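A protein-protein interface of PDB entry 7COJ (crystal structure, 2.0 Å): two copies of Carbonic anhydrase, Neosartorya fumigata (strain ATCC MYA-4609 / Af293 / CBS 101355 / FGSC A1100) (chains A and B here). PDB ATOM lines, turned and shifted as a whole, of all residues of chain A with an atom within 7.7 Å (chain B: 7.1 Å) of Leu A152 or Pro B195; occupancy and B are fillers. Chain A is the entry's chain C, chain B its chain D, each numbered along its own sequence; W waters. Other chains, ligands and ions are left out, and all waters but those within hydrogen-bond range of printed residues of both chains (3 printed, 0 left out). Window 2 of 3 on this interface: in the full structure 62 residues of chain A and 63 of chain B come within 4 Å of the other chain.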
ATOM      1  N   HIS A 140      20.943  25.682  -3.699  1.00  0.00           N
ATOM      2  CA  HIS A 140      20.599  24.358  -3.135  1.00  0.00           C
ATOM      3  C   HIS A 140      20.315  23.385  -4.295  1.00  0.00           C
ATOM      4  O   HIS A 140      19.510  23.700  -5.168  1.00  0.00           O
ATOM      5  CB  HIS A 140      19.441  24.498  -2.169  1.00  0.00           C
ATOM      6  CG  HIS A 140      19.097  23.255  -1.421  1.00  0.00           C
ATOM      7  ND1 HIS A 140      20.026  22.580  -0.643  1.00  0.00           N
ATOM      8  CD2 HIS A 140      17.942  22.552  -1.325  1.00  0.00           C
ATOM      9  CE1 HIS A 140      19.435  21.541  -0.054  1.00  0.00           C
ATOM     10  NE2 HIS A 140      18.161  21.507  -0.448  1.00  0.00           N
ATOM     11  N   HIS A 148      10.469  18.869  -0.074  1.00  0.00           N
ATOM     12  CA  HIS A 148       9.676  18.224   1.008  1.00  0.00           C
ATOM     13  C   HIS A 148       9.318  19.346   1.964  1.00  0.00           C
ATOM     14  O   HIS A 148      10.209  20.090   2.384  1.00  0.00           O
ATOM     15  CB  HIS A 148      10.447  17.126   1.738  1.00  0.00           C
ATOM     16  CG  HIS A 148      10.802  15.921   0.938  1.00  0.00           C
ATOM     17  ND1 HIS A 148      10.168  14.727   1.109  1.00  0.00           N
ATOM     18  CD2 HIS A 148      11.767  15.713   0.026  1.00  0.00           C
ATOM     19  CE1 HIS A 148      10.693  13.831   0.312  1.00  0.00           C
ATOM     20  NE2 HIS A 148      11.688  14.412  -0.398  1.00  0.00           N
ATOM     21  N   PRO A 149       8.021  19.592   2.255  1.00  0.00           N
ATOM     22  CA  PRO A 149       7.647  20.741   3.088  1.00  0.00           C
ATOM     23  C   PRO A 149       8.438  20.855   4.415  1.00  0.00           C
ATOM     24  O   PRO A 149       8.809  21.935   4.778  1.00  0.00           O
ATOM     25  CB  PRO A 149       6.156  20.483   3.347  1.00  0.00           C
ATOM     26  CG  PRO A 149       5.703  19.741   2.100  1.00  0.00           C
ATOM     27  CD  PRO A 149       6.866  18.829   1.758  1.00  0.00           C
ATOM     28  N   ALA A 150       8.711  19.735   5.080  1.00  0.00           N
ATOM     29  CA  ALA A 150       9.320  19.699   6.423  1.00  0.00           C
ATOM     30  C   ALA A 150      10.802  19.312   6.370  1.00  0.00           C
ATOM     31  O   ALA A 150      11.367  19.057   7.454  1.00  0.00           O
ATOM     32  CB  ALA A 150       8.558  18.722   7.278  1.00  0.00           C
ATOM     33  N   ASP A 151      11.432  19.345   5.185  1.00  0.00           N
ATOM     34  CA  ASP A 151      12.877  19.070   4.994  1.00  0.00           C
ATOM     35  C   ASP A 151      13.687  20.218   5.621  1.00  0.00           C
ATOM     36  O   ASP A 151      13.494  21.365   5.175  1.00  0.00           O
ATOM     37  CB  ASP A 151      13.178  18.889   3.501  1.00  0.00           C
ATOM     38  CG  ASP A 151      14.659  18.771   3.165  1.00  0.00           C
ATOM     39  OD1 ASP A 151      15.379  18.249   3.973  1.00  0.00           O
ATOM     40  OD2 ASP A 151      15.066  19.271   2.115  1.00  0.00           O
ATOM     41  N   LEU A 152      14.585  19.942   6.580  1.00  0.00           N
ATOM     42  CA  LEU A 152      15.409  21.008   7.210  1.00  0.00           C
ATOM     43  C   LEU A 152      16.466  21.528   6.243  1.00  0.00           C
ATOM     44  O   LEU A 152      16.860  22.655   6.399  1.00  0.00           O
ATOM     45  CB  LEU A 152      16.118  20.498   8.472  1.00  0.00           C
ATOM     46  CG  LEU A 152      15.238  20.364   9.710  1.00  0.00           C
ATOM     47  CD1 LEU A 152      16.100  19.962  10.895  1.00  0.00           C
ATOM     48  CD2 LEU A 152      14.494  21.666   9.998  1.00  0.00           C
ATOM     49  N   SER A 153      16.977  20.690   5.356  1.00  0.00           N
ATOM     50  CA  SER A 153      18.071  21.058   4.427  1.00  0.00           C
ATOM     51  C   SER A 153      17.606  22.194   3.506  1.00  0.00           C
ATOM     52  O   SER A 153      18.205  23.284   3.527  1.00  0.00           O
ATOM     53  CB  SER A 153      18.522  19.860   3.663  1.00  0.00           C
ATOM     54  OG  SER A 153      19.616  20.188   2.824  1.00  0.00           O
ATOM     55  N   SER A 154      16.502  22.005   2.777  1.00  0.00           N
ATOM     56  CA  SER A 154      15.934  23.059   1.922  1.00  0.00           C
ATOM     57  C   SER A 154      15.323  24.158   2.808  1.00  0.00           C
ATOM     58  O   SER A 154      15.441  25.352   2.448  1.00  0.00           O
ATOM     59  CB  SER A 154      14.937  22.499   0.920  1.00  0.00           C
ATOM     60  OG  SER A 154      13.813  21.962   1.601  1.00  0.00           O
ATOM     61  N   GLY A 155      14.703  23.791   3.919  1.00  0.00           N
ATOM     62  CA  GLY A 155      14.094  24.758   4.847  1.00  0.00           C
ATOM     63  C   GLY A 155      15.096  25.787   5.349  1.00  0.00           C
ATOM     64  O   GLY A 155      14.782  27.010   5.383  1.00  0.00           O
ATOM     65  N   ALA A 156      16.274  25.320   5.769  1.00  0.00           N
ATOM     66  CA  ALA A 156      17.323  26.209   6.303  1.00  0.00           C
ATOM     67  C   ALA A 156      17.835  27.109   5.175  1.00  0.00           C
ATOM     68  O   ALA A 156      18.068  28.324   5.425  1.00  0.00           O
ATOM     69  CB  ALA A 156      18.425  25.393   6.932  1.00  0.00           C
ATOM     70  N   VAL A 157      18.021  26.579   3.960  1.00  0.00           N
ATOM     71  CA  VAL A 157      18.536  27.469   2.888  1.00  0.00           C
ATOM     72  C   VAL A 157      17.509  28.546   2.567  1.00  0.00           C
ATOM     73  O   VAL A 157      17.946  29.696   2.374  1.00  0.00           O
ATOM     74  CB  VAL A 157      19.159  26.841   1.629  1.00  0.00           C
ATOM     75  CG1 VAL A 157      19.726  25.468   1.791  1.00  0.00           C
ATOM     76  CG2 VAL A 157      18.443  27.104   0.324  1.00  0.00           C
ATOM     77  N   ILE A 158      16.225  28.204   2.532  1.00  0.00           N
ATOM     78  CA  ILE A 158      15.155  29.177   2.183  1.00  0.00           C
ATOM     79  C   ILE A 158      15.103  30.254   3.277  1.00  0.00           C
ATOM     80  O   ILE A 158      15.119  31.439   2.933  1.00  0.00           O
ATOM     81  CB  ILE A 158      13.826  28.452   1.936  1.00  0.00           C
ATOM     82  CG1 ILE A 158      13.921  27.600   0.665  1.00  0.00           C
ATOM     83  CG2 ILE A 158      12.676  29.438   1.844  1.00  0.00           C
ATOM     84  CD1 ILE A 158      12.852  26.538   0.545  1.00  0.00           C
ATOM     85  N   GLU A 159      15.078  29.862   4.543  1.00  0.00           N
ATOM     86  CA  GLU A 159      15.064  30.820   5.677  1.00  0.00           C
ATOM     87  C   GLU A 159      16.245  31.789   5.527  1.00  0.00           C
ATOM     88  O   GLU A 159      16.038  33.007   5.623  1.00  0.00           O
ATOM     89  CB  GLU A 159      15.120  30.051   7.002  1.00  0.00           C
ATOM     90  CG  GLU A 159      15.321  30.922   8.245  1.00  0.00           C
ATOM     91  CD  GLU A 159      14.145  31.828   8.579  1.00  0.00           C
ATOM     92  OE1 GLU A 159      13.040  31.595   8.024  1.00  0.00           O
ATOM     93  OE2 GLU A 159      14.355  32.793   9.392  1.00  0.00           O
ATOM     94  N   LYS A 238       5.527  28.709   2.963  1.00  0.00           N
ATOM     95  CA  LYS A 238       6.458  29.049   4.062  1.00  0.00           C
ATOM     96  C   LYS A 238       6.242  30.519   4.406  1.00  0.00           C
ATOM     97  O   LYS A 238       6.336  31.323   3.488  1.00  0.00           O
ATOM     98  CB  LYS A 238       7.884  28.750   3.601  1.00  0.00           C
ATOM     99  CG  LYS A 238       8.134  27.292   3.275  1.00  0.00           C
ATOM    100  CD  LYS A 238       9.469  27.077   2.676  1.00  0.00           C
ATOM    101  CE  LYS A 238       9.732  25.647   2.268  1.00  0.00           C
ATOM    102  NZ  LYS A 238       9.504  24.665   3.357  1.00  0.00           N
ATOM    103  N   ILE B 143      23.456  24.556   3.731  1.00  0.00           N
ATOM    104  CA  ILE B 143      24.069  25.545   4.650  1.00  0.00           C
ATOM    105  C   ILE B 143      25.251  24.881   5.367  1.00  0.00           C
ATOM    106  O   ILE B 143      25.031  23.943   6.150  1.00  0.00           O
ATOM    107  CB  ILE B 143      23.063  26.085   5.673  1.00  0.00           C
ATOM    108  CG1 ILE B 143      21.868  26.783   5.023  1.00  0.00           C
ATOM    109  CG2 ILE B 143      23.769  26.994   6.668  1.00  0.00           C
ATOM    110  CD1 ILE B 143      22.240  28.002   4.267  1.00  0.00           C
ATOM    111  N   HIS B 148      24.334  15.681   8.140  1.00  0.00           N
ATOM    112  CA  HIS B 148      23.538  15.057   9.224  1.00  0.00           C
ATOM    113  C   HIS B 148      23.453  13.594   8.841  1.00  0.00           C
ATOM    114  O   HIS B 148      23.079  13.276   7.708  1.00  0.00           O
ATOM    115  CB  HIS B 148      22.152  15.689   9.382  1.00  0.00           C
ATOM    116  CG  HIS B 148      22.124  17.110   9.840  1.00  0.00           C
ATOM    117  ND1 HIS B 148      21.755  17.474  11.106  1.00  0.00           N
ATOM    118  CD2 HIS B 148      22.366  18.262   9.193  1.00  0.00           C
ATOM    119  CE1 HIS B 148      21.756  18.785  11.219  1.00  0.00           C
ATOM    120  NE2 HIS B 148      22.145  19.304  10.046  1.00  0.00           N
ATOM    121  N   ASP B 151      20.034  12.525   7.409  1.00  0.00           N
ATOM    122  CA  ASP B 151      19.414  13.483   6.449  1.00  0.00           C
ATOM    123  C   ASP B 151      19.105  12.740   5.139  1.00  0.00           C
ATOM    124  O   ASP B 151      20.037  12.207   4.546  1.00  0.00           O
ATOM    125  CB  ASP B 151      20.356  14.672   6.256  1.00  0.00           C
ATOM    126  CG  ASP B 151      19.944  15.642   5.169  1.00  0.00           C
ATOM    127  OD1 ASP B 151      18.760  15.807   4.980  1.00  0.00           O
ATOM    128  OD2 ASP B 151      20.829  16.179   4.493  1.00  0.00           O
ATOM    129  N   LEU B 190      17.962  31.377  15.753  1.00  0.00           N
ATOM    130  CA  LEU B 190      17.849  31.659  14.295  1.00  0.00           C
ATOM    131  C   LEU B 190      16.686  30.863  13.670  1.00  0.00           C
ATOM    132  O   LEU B 190      16.690  30.660  12.438  1.00  0.00           O
ATOM    133  CB  LEU B 190      19.190  31.307  13.644  1.00  0.00           C
ATOM    134  CG  LEU B 190      20.354  32.195  14.071  1.00  0.00           C
ATOM    135  CD1 LEU B 190      21.697  31.534  13.790  1.00  0.00           C
ATOM    136  CD2 LEU B 190      20.269  33.570  13.425  1.00  0.00           C
ATOM    137  N   GLY B 191      15.733  30.428  14.487  1.00  0.00           N
ATOM    138  CA  GLY B 191      14.542  29.696  14.031  1.00  0.00           C
ATOM    139  C   GLY B 191      14.919  28.349  13.432  1.00  0.00           C
ATOM    140  O   GLY B 191      15.663  27.623  14.073  1.00  0.00           O
ATOM    141  N   ILE B 192      14.469  28.044  12.204  1.00  0.00           N
ATOM    142  CA  ILE B 192      14.636  26.676  11.627  1.00  0.00           C
ATOM    143  C   ILE B 192      16.129  26.387  11.386  1.00  0.00           C
ATOM    144  O   ILE B 192      16.521  25.191  11.281  1.00  0.00           O
ATOM    145  CB  ILE B 192      13.767  26.525  10.364  1.00  0.00           C
ATOM    146  CG1 ILE B 192      13.545  25.048  10.012  1.00  0.00           C
ATOM    147  CG2 ILE B 192      14.341  27.329   9.204  1.00  0.00           C
ATOM    148  CD1 ILE B 192      12.597  24.832   8.834  1.00  0.00           C
ATOM    149  N   LEU B 193      16.968  27.426  11.335  1.00  0.00           N
ATOM    150  CA  LEU B 193      18.445  27.253  11.212  1.00  0.00           C
ATOM    151  C   LEU B 193      19.034  26.557  12.448  1.00  0.00           C
ATOM    152  O   LEU B 193      20.097  25.896  12.274  1.00  0.00           O
ATOM    153  CB  LEU B 193      19.093  28.614  10.951  1.00  0.00           C
ATOM    154  CG  LEU B 193      18.946  29.084   9.501  1.00  0.00           C
ATOM    155  CD1 LEU B 193      19.045  30.593   9.375  1.00  0.00           C
ATOM    156  CD2 LEU B 193      20.001  28.437   8.624  1.00  0.00           C
ATOM    157  N   ASP B 194      18.384  26.645  13.629  1.00  0.00           N
ATOM    158  CA  ASP B 194      18.975  26.123  14.898  1.00  0.00           C
ATOM    159  C   ASP B 194      19.184  24.613  14.800  1.00  0.00           C
ATOM    160  O   ASP B 194      20.299  24.118  15.002  1.00  0.00           O
ATOM    161  CB  ASP B 194      18.176  26.500  16.146  1.00  0.00           C
ATOM    162  CG  ASP B 194      18.225  27.990  16.497  1.00  0.00           C
ATOM    163  OD1 ASP B 194      19.058  28.742  15.898  1.00  0.00           O
ATOM    164  OD2 ASP B 194      17.402  28.404  17.332  1.00  0.00           O
ATOM    165  N   PRO B 195      18.148  23.794  14.479  1.00  0.00           N
ATOM    166  CA  PRO B 195      18.373  22.349  14.404  1.00  0.00           C
ATOM    167  C   PRO B 195      19.361  22.001  13.282  1.00  0.00           C
ATOM    168  O   PRO B 195      20.119  21.065  13.448  1.00  0.00           O
ATOM    169  CB  PRO B 195      16.968  21.756  14.180  1.00  0.00           C
ATOM    170  CG  PRO B 195      16.127  22.937  13.696  1.00  0.00           C
ATOM    171  CD  PRO B 195      16.719  24.156  14.368  1.00  0.00           C
ATOM    172  N   TRP B 196      19.348  22.759  12.182  1.00  0.00           N
ATOM    173  CA  TRP B 196      20.264  22.502  11.043  1.00  0.00           C
ATOM    174  C   TRP B 196      21.723  22.630  11.503  1.00  0.00           C
ATOM    175  O   TRP B 196      22.550  21.836  11.064  1.00  0.00           O
ATOM    176  CB  TRP B 196      19.994  23.436   9.867  1.00  0.00           C
ATOM    177  CG  TRP B 196      20.930  23.099   8.756  1.00  0.00           C
ATOM    178  CD1 TRP B 196      22.070  23.762   8.415  1.00  0.00           C
ATOM    179  CD2 TRP B 196      20.903  21.894   7.975  1.00  0.00           C
ATOM    180  NE1 TRP B 196      22.725  23.072   7.445  1.00  0.00           N
ATOM    181  CE2 TRP B 196      22.033  21.928   7.146  1.00  0.00           C
ATOM    182  CE3 TRP B 196      19.998  20.833   7.853  1.00  0.00           C
ATOM    183  CZ2 TRP B 196      22.297  20.939   6.204  1.00  0.00           C
ATOM    184  CZ3 TRP B 196      20.285  19.816   6.954  1.00  0.00           C
ATOM    185  CH2 TRP B 196      21.403  19.893   6.116  1.00  0.00           C
ATOM    186  N   LEU B 197      22.028  23.595  12.358  1.00  0.00           N
ATOM    187  CA  LEU B 197      23.434  23.902  12.744  1.00  0.00           C
ATOM    188  C   LEU B 197      23.880  23.062  13.944  1.00  0.00           C
ATOM    189  O   LEU B 197      25.077  23.180  14.350  1.00  0.00           O
ATOM    190  CB  LEU B 197      23.547  25.398  13.042  1.00  0.00           C
ATOM    191  CG  LEU B 197      23.324  26.319  11.844  1.00  0.00           C
ATOM    192  CD1 LEU B 197      23.289  27.763  12.292  1.00  0.00           C
ATOM    193  CD2 LEU B 197      24.359  26.123  10.761  1.00  0.00           C
ATOM    194  N   ILE B 198      23.024  22.198  14.491  1.00  0.00           N
ATOM    195  CA  ILE B 198      23.392  21.413  15.697  1.00  0.00           C
ATOM    196  C   ILE B 198      24.738  20.693  15.513  1.00  0.00           C
ATOM    197  O   ILE B 198      25.524  20.640  16.446  1.00  0.00           O
ATOM    198  CB  ILE B 198      22.268  20.435  16.093  1.00  0.00           C
ATOM    199  CG1 ILE B 198      21.137  21.150  16.831  1.00  0.00           C
ATOM    200  CG2 ILE B 198      22.816  19.301  16.940  1.00  0.00           C
ATOM    201  CD1 ILE B 198      19.901  20.271  17.020  1.00  0.00           C
ATOM    202  N   PRO B 199      25.049  20.034  14.383  1.00  0.00           N
ATOM    203  CA  PRO B 199      26.320  19.320  14.259  1.00  0.00           C
ATOM    204  C   PRO B 199      27.550  20.221  14.448  1.00  0.00           C
ATOM    205  O   PRO B 199      28.549  19.739  14.962  1.00  0.00           O
ATOM    206  CB  PRO B 199      26.269  18.683  12.862  1.00  0.00           C
ATOM    207  CG  PRO B 199      24.763  18.531  12.616  1.00  0.00           C
ATOM    208  CD  PRO B 199      24.182  19.805  13.214  1.00  0.00           C
HETATM  209  O   HOH W   1      16.619  32.883  10.859  1.00  0.00           O
HETATM  210  O   HOH W   2      20.779  23.565   4.534  1.00  0.00           O
HETATM  211  O   HOH W   3      21.487  18.268   3.047  1.00  0.00           O
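OD1 of Asp A151 is in hydrogen-bond range of N of Ser A153, 3.2 Å away.
O of Ile B143 is in hydrogen-bond range of NE1 of Trp B196 (2.8 Å).
NE2 of His B148 is in hydrogen-bond range of O of Trp B196 (2.8 Å).
Among the printed residues, pairs that only touch across the chains: Leu A152 with Ile B192, Ser A153 with Trp B196, Glu A159 with Ile B192, Ala A156 with Leu B193, Leu A152 with Pro B195, Ala A156 with Trp B196, Gly A155 with Ile B192, Glu A159 with Leu B193, Leu A152 with Trp B196 and Val A157 with Ile B143.
Leu A152 touches just these residues of chain B: Ile B192 (3.5 Å), Pro B195 (3.8 Å) and Trp B196 (3.9 Å).
Of the printed residues of chain A, Pro B195 touches Leu A152.
Of the printed residues of chain B, Val A157 touches Ile B143.
Printed residues of chain A within 4 Å of Ile B192: Leu A152, Gly A155 and Glu A159.
Of the printed residues of chain A, Leu B193 touches Ala A156 (3.7 Å) and Glu A159 (3.9 Å).
Of the printed residues of chain B, Glu A159 touches Ile B192 and Leu B193.
Of the printed residues of chain B, Ser A153 touches Trp B196 (3.6 Å).
His B148 touches none of the printed residues of chain A.
The nearest residue of chain B that does not touch Leu A152 is His B148 (5.8 Å).
The nearest residue of chain A that does not touch Pro B195 is Ala A156 (7.3 Å).
The nearest printed residue of chain A that does not touch Ile B143 is Ala A156 (4.05 Å).
Of the 13 printed residues of chain B, 5 touch a printed residue of chain A.
Printed residues of chain B that touch a printed residue of chain A: Ile B143, Ile B192, Leu B193, Pro B195 and Trp B196.
Hydrophobic or aromatic side chains of chain B that line the printed part of chain A: Ile B143, Ile B192, Leu B193, Pro B195 and Trp B196.
Of the 14 printed residues of chain A, 6 touch a printed residue of chain B.
Printed residues of chain A that touch a printed residue of chain B: Leu A152, Ser A153, Gly A155, Ala A156, Val A157 and Glu A159.
Hydrophobic or aromatic side chains of chain A within 4 Å of the printed part of chain B: Leu A152 and Ala A156.
Positions printed for both chains: 148 and 151.
Water W3 lies within hydrogen-bond range of OD2 of Asp B151 (2.6 Å) and OG of Ser A153 (2.7 Å).
Water W1 bridges OE2 of Glu A159 (2.7 Å) and O of Leu B190 (2.7 Å).
Water W2 bridges O of Ser A153 (2.8 Å) and N of Ile B143 (3.0 Å).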
